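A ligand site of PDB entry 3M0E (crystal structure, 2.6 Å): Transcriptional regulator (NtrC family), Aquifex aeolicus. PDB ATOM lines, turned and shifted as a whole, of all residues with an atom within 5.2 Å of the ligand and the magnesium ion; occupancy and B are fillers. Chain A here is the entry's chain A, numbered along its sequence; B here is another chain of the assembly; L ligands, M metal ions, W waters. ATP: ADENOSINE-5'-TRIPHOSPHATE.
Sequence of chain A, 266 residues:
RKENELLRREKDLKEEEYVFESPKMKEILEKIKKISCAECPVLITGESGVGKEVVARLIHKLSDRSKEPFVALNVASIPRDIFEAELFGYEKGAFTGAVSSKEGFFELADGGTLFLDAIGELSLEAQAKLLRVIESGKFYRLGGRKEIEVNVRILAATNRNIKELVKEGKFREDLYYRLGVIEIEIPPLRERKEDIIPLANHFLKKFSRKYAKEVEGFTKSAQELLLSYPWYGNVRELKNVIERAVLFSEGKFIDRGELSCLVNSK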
ATOM      1  N   GLU A  17     -37.590   3.286   5.326  1.00  0.00           N
ATOM      2  CA  GLU A  17     -36.258   3.856   5.544  1.00  0.00           C
ATOM      3  C   GLU A  17     -35.157   3.007   4.935  1.00  0.00           C
ATOM      4  O   GLU A  17     -33.981   3.143   5.295  1.00  0.00           O
ATOM      5  CB  GLU A  17     -35.984   4.071   7.044  1.00  0.00           C
ATOM      6  CG  GLU A  17     -35.520   2.807   7.791  1.00  0.00           C
ATOM      7  CD  GLU A  17     -36.668   1.888   8.182  1.00  0.00           C
ATOM      8  OE1 GLU A  17     -37.810   2.109   7.719  1.00  0.00           O
ATOM      9  OE2 GLU A  17     -36.428   0.932   8.947  1.00  0.00           O
ATOM     10  N   TYR A  18     -35.519   2.103   4.028  1.00  0.00           N
ATOM     11  CA  TYR A  18     -34.522   1.346   3.283  1.00  0.00           C
ATOM     12  C   TYR A  18     -34.343   1.926   1.890  1.00  0.00           C
ATOM     13  O   TYR A  18     -35.299   2.430   1.306  1.00  0.00           O
ATOM     14  CB  TYR A  18     -34.843  -0.167   3.262  1.00  0.00           C
ATOM     15  CG  TYR A  18     -34.612  -0.801   4.618  1.00  0.00           C
ATOM     16  CD1 TYR A  18     -35.662  -1.374   5.338  1.00  0.00           C
ATOM     17  CD2 TYR A  18     -33.343  -0.769   5.209  1.00  0.00           C
ATOM     18  CE1 TYR A  18     -35.434  -1.933   6.602  1.00  0.00           C
ATOM     19  CE2 TYR A  18     -33.094  -1.310   6.465  1.00  0.00           C
ATOM     20  CZ  TYR A  18     -34.141  -1.886   7.161  1.00  0.00           C
ATOM     21  OH  TYR A  18     -33.876  -2.424   8.418  1.00  0.00           O
ATOM     22  N   VAL A  19     -33.130   1.868   1.376  1.00  0.00           N
ATOM     23  CA  VAL A  19     -32.809   2.468   0.088  1.00  0.00           C
ATOM     24  C   VAL A  19     -32.724   1.462  -1.061  1.00  0.00           C
ATOM     25  O   VAL A  19     -31.904   0.530  -1.048  1.00  0.00           O
ATOM     26  CB  VAL A  19     -31.480   3.216   0.167  1.00  0.00           C
ATOM     27  CG1 VAL A  19     -31.003   3.609  -1.218  1.00  0.00           C
ATOM     28  CG2 VAL A  19     -31.604   4.431   1.084  1.00  0.00           C
ATOM     29  N   PHE A  20     -33.574   1.656  -2.063  1.00  0.00           N
ATOM     30  CA  PHE A  20     -33.532   0.850  -3.281  1.00  0.00           C
ATOM     31  C   PHE A  20     -33.610   1.780  -4.498  1.00  0.00           C
ATOM     32  O   PHE A  20     -34.697   2.242  -4.868  1.00  0.00           O
ATOM     33  CB  PHE A  20     -34.710  -0.118  -3.333  1.00  0.00           C
ATOM     34  CG  PHE A  20     -34.772  -1.068  -2.167  1.00  0.00           C
ATOM     35  CD1 PHE A  20     -35.425  -0.717  -0.994  1.00  0.00           C
ATOM     36  CD2 PHE A  20     -34.210  -2.343  -2.264  1.00  0.00           C
ATOM     37  CE1 PHE A  20     -35.498  -1.610   0.074  1.00  0.00           C
ATOM     38  CE2 PHE A  20     -34.283  -3.235  -1.197  1.00  0.00           C
ATOM     39  CZ  PHE A  20     -34.939  -2.871  -0.025  1.00  0.00           C
ATOM     40  N   GLY A  46     -25.695 -13.522  -1.834  1.00  0.00           N
ATOM     41  CA  GLY A  46     -24.896 -12.335  -2.090  1.00  0.00           C
ATOM     42  C   GLY A  46     -23.777 -12.153  -1.072  1.00  0.00           C
ATOM     43  O   GLY A  46     -23.790 -12.718   0.018  1.00  0.00           O
ATOM     44  N   GLU A  47     -22.783 -11.349  -1.440  1.00  0.00           N
ATOM     45  CA  GLU A  47     -21.654 -11.053  -0.566  1.00  0.00           C
ATOM     46  C   GLU A  47     -22.059 -10.472   0.771  1.00  0.00           C
ATOM     47  O   GLU A  47     -23.176  -9.932   0.926  1.00  0.00           O
ATOM     48  CB  GLU A  47     -20.726 -10.056  -1.242  1.00  0.00           C
ATOM     49  CG  GLU A  47     -20.100 -10.555  -2.509  1.00  0.00           C
ATOM     50  CD  GLU A  47     -19.081  -9.559  -3.057  1.00  0.00           C
ATOM     51  OE1 GLU A  47     -18.848  -8.523  -2.384  1.00  0.00           O
ATOM     52  OE2 GLU A  47     -18.526  -9.803  -4.153  1.00  0.00           O
ATOM     53  N   SER A  48     -21.122 -10.553   1.718  1.00  0.00           N
ATOM     54  CA  SER A  48     -21.345  -9.994   3.050  1.00  0.00           C
ATOM     55  C   SER A  48     -21.699  -8.503   2.989  1.00  0.00           C
ATOM     56  O   SER A  48     -20.999  -7.709   2.376  1.00  0.00           O
ATOM     57  CB  SER A  48     -20.106 -10.188   3.907  1.00  0.00           C
ATOM     58  OG  SER A  48     -20.282  -9.549   5.163  1.00  0.00           O
ATOM     59  N   GLY A  49     -22.803  -8.131   3.619  1.00  0.00           N
ATOM     60  CA  GLY A  49     -23.183  -6.740   3.716  1.00  0.00           C
ATOM     61  C   GLY A  49     -24.054  -6.203   2.591  1.00  0.00           C
ATOM     62  O   GLY A  49     -24.308  -4.991   2.526  1.00  0.00           O
ATOM     63  N   VAL A  50     -24.537  -7.071   1.702  1.00  0.00           N
ATOM     64  CA  VAL A  50     -25.323  -6.552   0.583  1.00  0.00           C
ATOM     65  C   VAL A  50     -26.777  -6.383   0.926  1.00  0.00           C
ATOM     66  O   VAL A  50     -27.529  -5.829   0.137  1.00  0.00           O
ATOM     67  CB  VAL A  50     -25.198  -7.399  -0.684  1.00  0.00           C
ATOM     68  CG1 VAL A  50     -23.725  -7.579  -1.077  1.00  0.00           C
ATOM     69  CG2 VAL A  50     -25.944  -8.720  -0.532  1.00  0.00           C
ATOM     70  N   GLY A  51     -27.194  -6.857   2.100  1.00  0.00           N
ATOM     71  CA  GLY A  51     -28.555  -6.672   2.586  1.00  0.00           C
ATOM     72  C   GLY A  51     -29.459  -7.903   2.609  1.00  0.00           C
ATOM     73  O   GLY A  51     -30.703  -7.800   2.513  1.00  0.00           O
ATOM     74  N   LYS A  52     -28.858  -9.098   2.730  1.00  0.00           N
ATOM     75  CA  LYS A  52     -29.667 -10.305   2.678  1.00  0.00           C
ATOM     76  C   LYS A  52     -30.684 -10.351   3.821  1.00  0.00           C
ATOM     77  O   LYS A  52     -31.855 -10.642   3.603  1.00  0.00           O
ATOM     78  CB  LYS A  52     -28.802 -11.558   2.678  1.00  0.00           C
ATOM     79  CG  LYS A  52     -27.851 -11.610   1.502  1.00  0.00           C
ATOM     80  CD  LYS A  52     -26.967 -12.864   1.570  1.00  0.00           C
ATOM     81  CE  LYS A  52     -26.027 -12.842   2.746  1.00  0.00           C
ATOM     82  NZ  LYS A  52     -24.957 -11.877   2.499  1.00  0.00           N
ATOM     83  N   GLU A  53     -30.242 -10.024   5.035  1.00  0.00           N
ATOM     84  CA  GLU A  53     -31.129 -10.013   6.184  1.00  0.00           C
ATOM     85  C   GLU A  53     -32.202  -8.912   6.070  1.00  0.00           C
ATOM     86  O   GLU A  53     -33.338  -9.106   6.484  1.00  0.00           O
ATOM     87  CB  GLU A  53     -30.331  -9.831   7.468  1.00  0.00           C
ATOM     88  CG  GLU A  53     -31.208  -9.676   8.709  1.00  0.00           C
ATOM     89  CD  GLU A  53     -30.942 -10.742   9.766  1.00  0.00           C
ATOM     90  OE1 GLU A  53     -29.993 -11.550   9.591  1.00  0.00           O
ATOM     91  OE2 GLU A  53     -31.686 -10.751  10.773  1.00  0.00           O
ATOM     92  N   VAL A  54     -31.830  -7.761   5.522  1.00  0.00           N
ATOM     93  CA  VAL A  54     -32.825  -6.734   5.275  1.00  0.00           C
ATOM     94  C   VAL A  54     -33.899  -7.275   4.335  1.00  0.00           C
ATOM     95  O   VAL A  54     -35.106  -7.189   4.608  1.00  0.00           O
ATOM     96  CB  VAL A  54     -32.196  -5.494   4.684  1.00  0.00           C
ATOM     97  CG1 VAL A  54     -33.283  -4.544   4.215  1.00  0.00           C
ATOM     98  CG2 VAL A  54     -31.300  -4.839   5.714  1.00  0.00           C
ATOM     99  N   ASP A 117     -30.332 -18.875   8.244  1.00  0.00           N
ATOM    100  CA  ASP A 117     -29.180 -18.086   7.852  1.00  0.00           C
ATOM    101  C   ASP A 117     -27.925 -18.963   7.735  1.00  0.00           C
ATOM    102  O   ASP A 117     -27.791 -19.981   8.423  1.00  0.00           O
ATOM    103  CB  ASP A 117     -28.993 -16.954   8.881  1.00  0.00           C
ATOM    104  CG  ASP A 117     -28.039 -15.872   8.425  1.00  0.00           C
ATOM    105  OD1 ASP A 117     -27.729 -15.838   7.213  1.00  0.00           O
ATOM    106  OD2 ASP A 117     -27.616 -15.049   9.289  1.00  0.00           O
ATOM    107  N   ASN A 159     -23.890 -16.161   2.132  1.00  0.00           N
ATOM    108  CA  ASN A 159     -22.926 -15.398   1.386  1.00  0.00           C
ATOM    109  C   ASN A 159     -21.939 -16.319   0.680  1.00  0.00           C
ATOM    110  O   ASN A 159     -20.889 -15.865   0.216  1.00  0.00           O
ATOM    111  CB  ASN A 159     -22.220 -14.349   2.272  1.00  0.00           C
ATOM    112  CG  ASN A 159     -21.538 -14.958   3.523  1.00  0.00           C
ATOM    113  OD1 ASN A 159     -20.856 -15.988   3.443  1.00  0.00           O
ATOM    114  ND2 ASN A 159     -21.716 -14.291   4.661  1.00  0.00           N
ATOM    115  N   ARG A 192     -23.793  -1.571  -8.101  1.00  0.00           N
ATOM    116  CA  ARG A 192     -25.056  -0.874  -7.852  1.00  0.00           C
ATOM    117  C   ARG A 192     -24.737   0.593  -7.574  1.00  0.00           C
ATOM    118  O   ARG A 192     -25.305   1.183  -6.646  1.00  0.00           O
ATOM    119  CB  ARG A 192     -25.770  -1.414  -6.617  1.00  0.00           C
ATOM    120  CG  ARG A 192     -26.223  -2.839  -6.706  1.00  0.00           C
ATOM    121  CD  ARG A 192     -26.229  -3.486  -5.314  1.00  0.00           C
ATOM    122  NE  ARG A 192     -27.024  -2.759  -4.324  1.00  0.00           N
ATOM    123  CZ  ARG A 192     -27.181  -3.171  -3.075  1.00  0.00           C
ATOM    124  NH1 ARG A 192     -26.593  -4.305  -2.690  1.00  0.00           N
ATOM    125  NH2 ARG A 192     -27.913  -2.478  -2.215  1.00  0.00           N
ATOM    126  N   LEU A 199     -27.384   5.920  -0.348  1.00  0.00           N
ATOM    127  CA  LEU A 199     -27.065   5.209   0.897  1.00  0.00           C
ATOM    128  C   LEU A 199     -26.209   6.090   1.824  1.00  0.00           C
ATOM    129  O   LEU A 199     -26.567   6.332   2.992  1.00  0.00           O
ATOM    130  CB  LEU A 199     -26.348   3.883   0.614  1.00  0.00           C
ATOM    131  CG  LEU A 199     -27.246   2.718   0.190  1.00  0.00           C
ATOM    132  CD1 LEU A 199     -26.428   1.620  -0.443  1.00  0.00           C
ATOM    133  CD2 LEU A 199     -28.061   2.206   1.355  1.00  0.00           C
ATOM    134  N   HIS A 202     -28.313   8.740   3.275  1.00  0.00           N
ATOM    135  CA  HIS A 202     -29.220   8.188   4.270  1.00  0.00           C
ATOM    136  C   HIS A 202     -28.514   8.002   5.608  1.00  0.00           C
ATOM    137  O   HIS A 202     -29.076   8.327   6.662  1.00  0.00           O
ATOM    138  CB  HIS A 202     -29.801   6.859   3.779  1.00  0.00           C
ATOM    139  CG  HIS A 202     -30.675   6.170   4.785  1.00  0.00           C
ATOM    140  ND1 HIS A 202     -30.245   5.080   5.521  1.00  0.00           N
ATOM    141  CD2 HIS A 202     -31.951   6.403   5.174  1.00  0.00           C
ATOM    142  CE1 HIS A 202     -31.221   4.669   6.309  1.00  0.00           C
ATOM    143  NE2 HIS A 202     -32.265   5.461   6.117  1.00  0.00           N
ATOM    144  N   PHE A 203     -27.280   7.510   5.578  1.00  0.00           N
ATOM    145  CA  PHE A 203     -26.543   7.267   6.822  1.00  0.00           C
ATOM    146  C   PHE A 203     -26.088   8.583   7.456  1.00  0.00           C
ATOM    147  O   PHE A 203     -26.223   8.787   8.666  1.00  0.00           O
ATOM    148  CB  PHE A 203     -25.341   6.332   6.620  1.00  0.00           C
ATOM    149  CG  PHE A 203     -25.731   4.942   6.207  1.00  0.00           C
ATOM    150  CD1 PHE A 203     -26.737   4.269   6.868  1.00  0.00           C
ATOM    151  CD2 PHE A 203     -25.081   4.314   5.138  1.00  0.00           C
ATOM    152  CE1 PHE A 203     -27.111   2.994   6.472  1.00  0.00           C
ATOM    153  CE2 PHE A 203     -25.434   3.051   4.747  1.00  0.00           C
ATOM    154  CZ  PHE A 203     -26.459   2.382   5.418  1.00  0.00           C
ATOM    155  N   VAL A 235     -22.797  -2.760   1.832  1.00  0.00           N
ATOM    156  CA  VAL A 235     -23.542  -1.725   2.537  1.00  0.00           C
ATOM    157  C   VAL A 235     -23.076  -1.530   3.986  1.00  0.00           C
ATOM    158  O   VAL A 235     -23.040  -0.403   4.486  1.00  0.00           O
ATOM    159  CB  VAL A 235     -25.064  -1.948   2.484  1.00  0.00           C
ATOM    160  CG1 VAL A 235     -25.797  -0.791   3.164  1.00  0.00           C
ATOM    161  CG2 VAL A 235     -25.505  -2.070   1.057  1.00  0.00           C
ATOM    162  N   ARG A 236     -22.677  -2.616   4.633  1.00  0.00           N
ATOM    163  CA  ARG A 236     -22.173  -2.524   6.007  1.00  0.00           C
ATOM    164  C   ARG A 236     -20.857  -1.755   6.103  1.00  0.00           C
ATOM    165  O   ARG A 236     -20.675  -0.912   6.987  1.00  0.00           O
ATOM    166  CB  ARG A 236     -22.045  -3.902   6.665  1.00  0.00           C
ATOM    167  CG  ARG A 236     -21.425  -3.825   8.031  1.00  0.00           C
ATOM    168  CD  ARG A 236     -21.290  -5.198   8.669  1.00  0.00           C
ATOM    169  NE  ARG A 236     -22.570  -5.767   9.041  1.00  0.00           N
ATOM    170  CZ  ARG A 236     -23.206  -6.704   8.347  1.00  0.00           C
ATOM    171  NH1 ARG A 236     -22.677  -7.183   7.221  1.00  0.00           N
ATOM    172  NH2 ARG A 236     -24.371  -7.163   8.780  1.00  0.00           N
ATOM    173  N   LYS A 239     -21.882   1.950   5.586  1.00  0.00           N
ATOM    174  CA  LYS A 239     -22.435   2.447   6.835  1.00  0.00           C
ATOM    175  C   LYS A 239     -21.367   2.685   7.916  1.00  0.00           C
ATOM    176  O   LYS A 239     -21.449   3.640   8.676  1.00  0.00           O
ATOM    177  CB  LYS A 239     -23.492   1.474   7.340  1.00  0.00           C
ATOM    178  CG  LYS A 239     -24.096   1.819   8.672  1.00  0.00           C
ATOM    179  CD  LYS A 239     -25.345   0.953   8.903  1.00  0.00           C
ATOM    180  CE  LYS A 239     -25.617   0.736  10.374  1.00  0.00           C
ATOM    181  NZ  LYS A 239     -24.355   0.310  11.086  1.00  0.00           N
ATOM    182  N   ARG B 132     -24.413 -13.525  14.825  1.00  0.00           N
ATOM    183  CA  ARG B 132     -25.707 -12.847  14.813  1.00  0.00           C
ATOM    184  C   ARG B 132     -25.875 -11.944  16.020  1.00  0.00           C
ATOM    185  O   ARG B 132     -26.651 -10.990  15.992  1.00  0.00           O
ATOM    186  CB  ARG B 132     -26.878 -13.829  14.701  1.00  0.00           C
ATOM    187  CG  ARG B 132     -26.868 -14.714  13.427  1.00  0.00           C
ATOM    188  CD  ARG B 132     -28.215 -15.426  13.256  1.00  0.00           C
ATOM    189  NE  ARG B 132     -29.305 -14.486  13.435  1.00  0.00           N
ATOM    190  CZ  ARG B 132     -29.806 -13.732  12.458  1.00  0.00           C
ATOM    191  NH1 ARG B 132     -29.314 -13.832  11.224  1.00  0.00           N
ATOM    192  NH2 ARG B 132     -30.794 -12.879  12.706  1.00  0.00           N
ATOM    193  N   GLU B 135     -24.595  -7.690  15.973  1.00  0.00           N
ATOM    194  CA  GLU B 135     -25.445  -6.598  15.497  1.00  0.00           C
ATOM    195  C   GLU B 135     -26.864  -6.618  16.059  1.00  0.00           C
ATOM    196  O   GLU B 135     -27.431  -5.566  16.300  1.00  0.00           O
ATOM    197  CB  GLU B 135     -25.447  -6.487  13.962  1.00  0.00           C
ATOM    198  CG  GLU B 135     -24.216  -5.754  13.361  1.00  0.00           C
ATOM    199  CD  GLU B 135     -24.313  -5.536  11.842  1.00  0.00           C
ATOM    200  OE1 GLU B 135     -25.270  -6.057  11.207  1.00  0.00           O
ATOM    201  OE2 GLU B 135     -23.429  -4.851  11.287  1.00  0.00           O
ATOM    202  N   ASP B 174     -17.407 -11.641   7.292  1.00  0.00           N
ATOM    203  CA  ASP B 174     -18.617 -11.047   7.841  1.00  0.00           C
ATOM    204  C   ASP B 174     -18.535 -10.668   9.329  1.00  0.00           C
ATOM    205  O   ASP B 174     -19.280  -9.804   9.792  1.00  0.00           O
ATOM    206  CB  ASP B 174     -19.891 -11.848   7.493  1.00  0.00           C
ATOM    207  CG  ASP B 174     -19.871 -13.323   7.966  1.00  0.00           C
ATOM    208  OD1 ASP B 174     -18.945 -13.739   8.711  1.00  0.00           O
ATOM    209  OD2 ASP B 174     -20.826 -14.058   7.587  1.00  0.00           O
ATOM    210  N   ARG B 178     -18.368  -6.640  11.133  1.00  0.00           N
ATOM    211  CA  ARG B 178     -19.260  -6.345  12.249  1.00  0.00           C
ATOM    212  C   ARG B 178     -18.482  -5.750  13.440  1.00  0.00           C
ATOM    213  O   ARG B 178     -18.988  -4.899  14.155  1.00  0.00           O
ATOM    214  CB  ARG B 178     -20.038  -7.583  12.690  1.00  0.00           C
ATOM    215  CG  ARG B 178     -21.221  -7.934  11.809  1.00  0.00           C
ATOM    216  CD  ARG B 178     -21.566  -9.393  11.965  1.00  0.00           C
ATOM    217  NE  ARG B 178     -22.863  -9.726  11.393  1.00  0.00           N
ATOM    218  CZ  ARG B 178     -23.045  -9.998  10.098  1.00  0.00           C
ATOM    219  NH1 ARG B 178     -22.013  -9.965   9.280  1.00  0.00           N
ATOM    220  NH2 ARG B 178     -24.254 -10.308   9.627  1.00  0.00           N
HETATM  221  PG  ATP L   1     -23.792 -10.738   5.972  1.00  0.00           P
HETATM  222  O1G ATP L   1     -23.478 -11.615   4.796  1.00  0.00           O
HETATM  223  O2G ATP L   1     -24.731 -11.344   6.991  1.00  0.00           O
HETATM  224  O3G ATP L   1     -22.535 -10.085   6.496  1.00  0.00           O
HETATM  225  PB  ATP L   1     -26.126  -9.320   4.870  1.00  0.00           P
HETATM  226  O1B ATP L   1     -27.154 -10.074   5.666  1.00  0.00           O
HETATM  227  O2B ATP L   1     -26.000  -9.503   3.392  1.00  0.00           O
HETATM  228  O3B ATP L   1     -24.618  -9.413   5.473  1.00  0.00           O
HETATM  229  PA  ATP L   1     -27.402  -7.144   6.214  1.00  0.00           P
HETATM  230  O1A ATP L   1     -26.987  -7.517   7.615  1.00  0.00           O
HETATM  231  O2A ATP L   1     -28.825  -7.439   5.799  1.00  0.00           O
HETATM  232  O3A ATP L   1     -26.360  -7.747   5.134  1.00  0.00           O
HETATM  233  O5' ATP L   1     -27.025  -5.584   6.062  1.00  0.00           O
HETATM  234  C5' ATP L   1     -25.774  -5.089   6.549  1.00  0.00           C
HETATM  235  C4' ATP L   1     -25.949  -3.650   7.039  1.00  0.00           C
HETATM  236  O4' ATP L   1     -26.275  -2.767   5.952  1.00  0.00           O
HETATM  237  C3' ATP L   1     -27.109  -3.602   8.001  1.00  0.00           C
HETATM  238  O3' ATP L   1     -26.847  -2.669   9.060  1.00  0.00           O
HETATM  239  C2' ATP L   1     -28.235  -3.073   7.147  1.00  0.00           C
HETATM  240  O2' ATP L   1     -29.198  -2.418   7.956  1.00  0.00           O
HETATM  241  C1' ATP L   1     -27.532  -2.145   6.176  1.00  0.00           C
HETATM  242  N9  ATP L   1     -28.297  -2.128   4.914  1.00  0.00           N
HETATM  243  C8  ATP L   1     -28.309  -3.133   4.035  1.00  0.00           C
HETATM  244  N7  ATP L   1     -29.100  -2.862   2.981  1.00  0.00           N
HETATM  245  C5  ATP L   1     -29.628  -1.652   3.195  1.00  0.00           C
HETATM  246  C6  ATP L   1     -30.539  -0.769   2.441  1.00  0.00           C
HETATM  247  N6  ATP L   1     -31.072  -1.178   1.240  1.00  0.00           N
HETATM  248  N1  ATP L   1     -30.817   0.427   3.006  1.00  0.00           N
HETATM  249  C2  ATP L   1     -30.303   0.794   4.190  1.00  0.00           C
HETATM  250  N3  ATP L   1     -29.467   0.047   4.926  1.00  0.00           N
HETATM  251  C4  ATP L   1     -29.088  -1.159   4.470  1.00  0.00           C
HETATM  252 MG    MG M   1     -27.038 -11.809   7.618  1.00  0.00          MG
HETATM  253  O   HOH W   1     -26.481 -13.869   6.082  1.00  0.00           O
HETATM  254  O   HOH W   2     -27.388  -9.614   9.591  1.00  0.00           O
HETATM  255  O   HOH W   3     -29.331  -3.577   0.093  1.00  0.00           O
HETATM  256  O   HOH W   4     -24.091 -13.834   8.206  1.00  0.00           O
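Water W2 lies within hydrogen-bond range of O1A of the ligand (2.9 Å), NH2 of Arg 178 of chain B (3.2 Å) and OE1 of Glu 53 (3.2 Å). Water W3 lies within hydrogen-bond range of the backbone carbonyl oxygen (O) of Val 50 (2.9 Å), the guanidinium group (NH2) of Arg 192 (2.9 Å) and a nitrogen (N7) of the ligand (3.0 Å).
The side-chain amino group (NZ) of Lys 52 is in hydrogen-bond range of the backbone carbonyl oxygen (O) of Glu 47, at 3.1 Å. The side-chain amino group of Lys 52 lies within hydrogen-bond range of the backbone carbonyl oxygen of Gly 46. The guanidinium group (NH1) of Arg 178 of chain B is in hydrogen-bond range of the backbone carbonyl oxygen (O) of Asp 174 of chain B, 2.8 Å away. The side-chain carboxylate (OE2) of Glu 135 of chain B lies within salt-bridge range of the guanidinium group (NE) of Arg 236 (2.6 Å). The backbone NH (N) of Val 235 lies within hydrogen-bond range of the backbone carbonyl oxygen (O) of Gly 49, 2.8 Å away. The side-chain amide nitrogen of Asn 159 sits at hydrogen-bond distance from the side-chain carboxylate of Asp 174 of chain B (3.1 Å). O of Val 50 lies within hydrogen-bond range of NH1 of Arg 192 (3.3 Å). The side-chain carboxylate of Asp 117 lies within salt-bridge range of the guanidinium group of Arg 132 of chain B (2.8 Å).
OE1 of Glu 53 touches the magnesium ion, at 3.6 Å. Asp 117 touches the magnesium ion. NH2 of Arg 178 of chain B touches the magnesium ion (3.7 Å). The nearest printed residue that does not touch the magnesium ion is Arg 132 of chain B (4.7 Å).
The side-chain hydroxyl of Ser 48 sits at hydrogen-bond distance from an oxygen (O3G) of the ligand (2.7 Å). O2B of the ligand lies within hydrogen-bond range of N of Lys 52. The side-chain amino group (NZ) of Lys 52 lies within salt-bridge range of an oxygen (O2B) of the ligand (2.7 Å). An oxygen (O3G) of the ligand is in salt-bridge range of the guanidinium group (NH1) of Arg 178 of chain B. NH2 of Arg 236 lies within salt-bridge range of O1A of the ligand, at 2.9 Å. An oxygen (O3B) of the ligand is in hydrogen-bond range of the backbone NH (N) of Gly 49 (2.9 Å). A nitrogen (N1) of the ligand is in hydrogen-bond range of the backbone NH (N) of Val 19, 3.2 Å away. The backbone carbonyl oxygen (O) of Val 19 lies within hydrogen-bond range of a nitrogen (N6) of the ligand, at 3.0 Å. O2A of the ligand sits at hydrogen-bond distance from N of Val 54, at 3.0 Å. N of Glu 53 is in hydrogen-bond range of O2A of the ligand, at 3.0 Å. The backbone NH (N) of Gly 51 is in hydrogen-bond range of an oxygen (O2B) of the ligand (3.2 Å). ND2 of Asn 159 lies within hydrogen-bond range of O1G of the ligand. An oxygen (O2B) of the ligand lies within hydrogen-bond range of the backbone NH (N) of Val 50, 3.3 Å away.
An oxygen (O2G) of the ligand binds the magnesium ion (2.4 Å). The magnesium ion has one donor atom within binding distance. Slightly farther from the magnesium ion lies O1B of the ligand (2.6 Å). Slightly farther from the magnesium ion lies water W1 (2.6 Å).
Tyr 18 touches the ligand. O of Glu 47 touches O2B of the ligand (3.8 Å). CD2 of Leu 199 touches N1 of the ligand, 3.7 Å away. Phe 203 touches the ligand (CZ to N3, 3.8 Å). CG1 of Val 235 touches N9 of the ligand, at 3.3 Å. Lys 239 touches the ligand. CB of Asp 174 of chain B touches O3G of the ligand, at 3.3 Å. Hydrophobic or aromatic side chains that line the ligand: Tyr 18, Val 54, Leu 199, Phe 203 and Val 235. Along chain A the residues within 4 Å of the ligand span positions 18 to 239.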
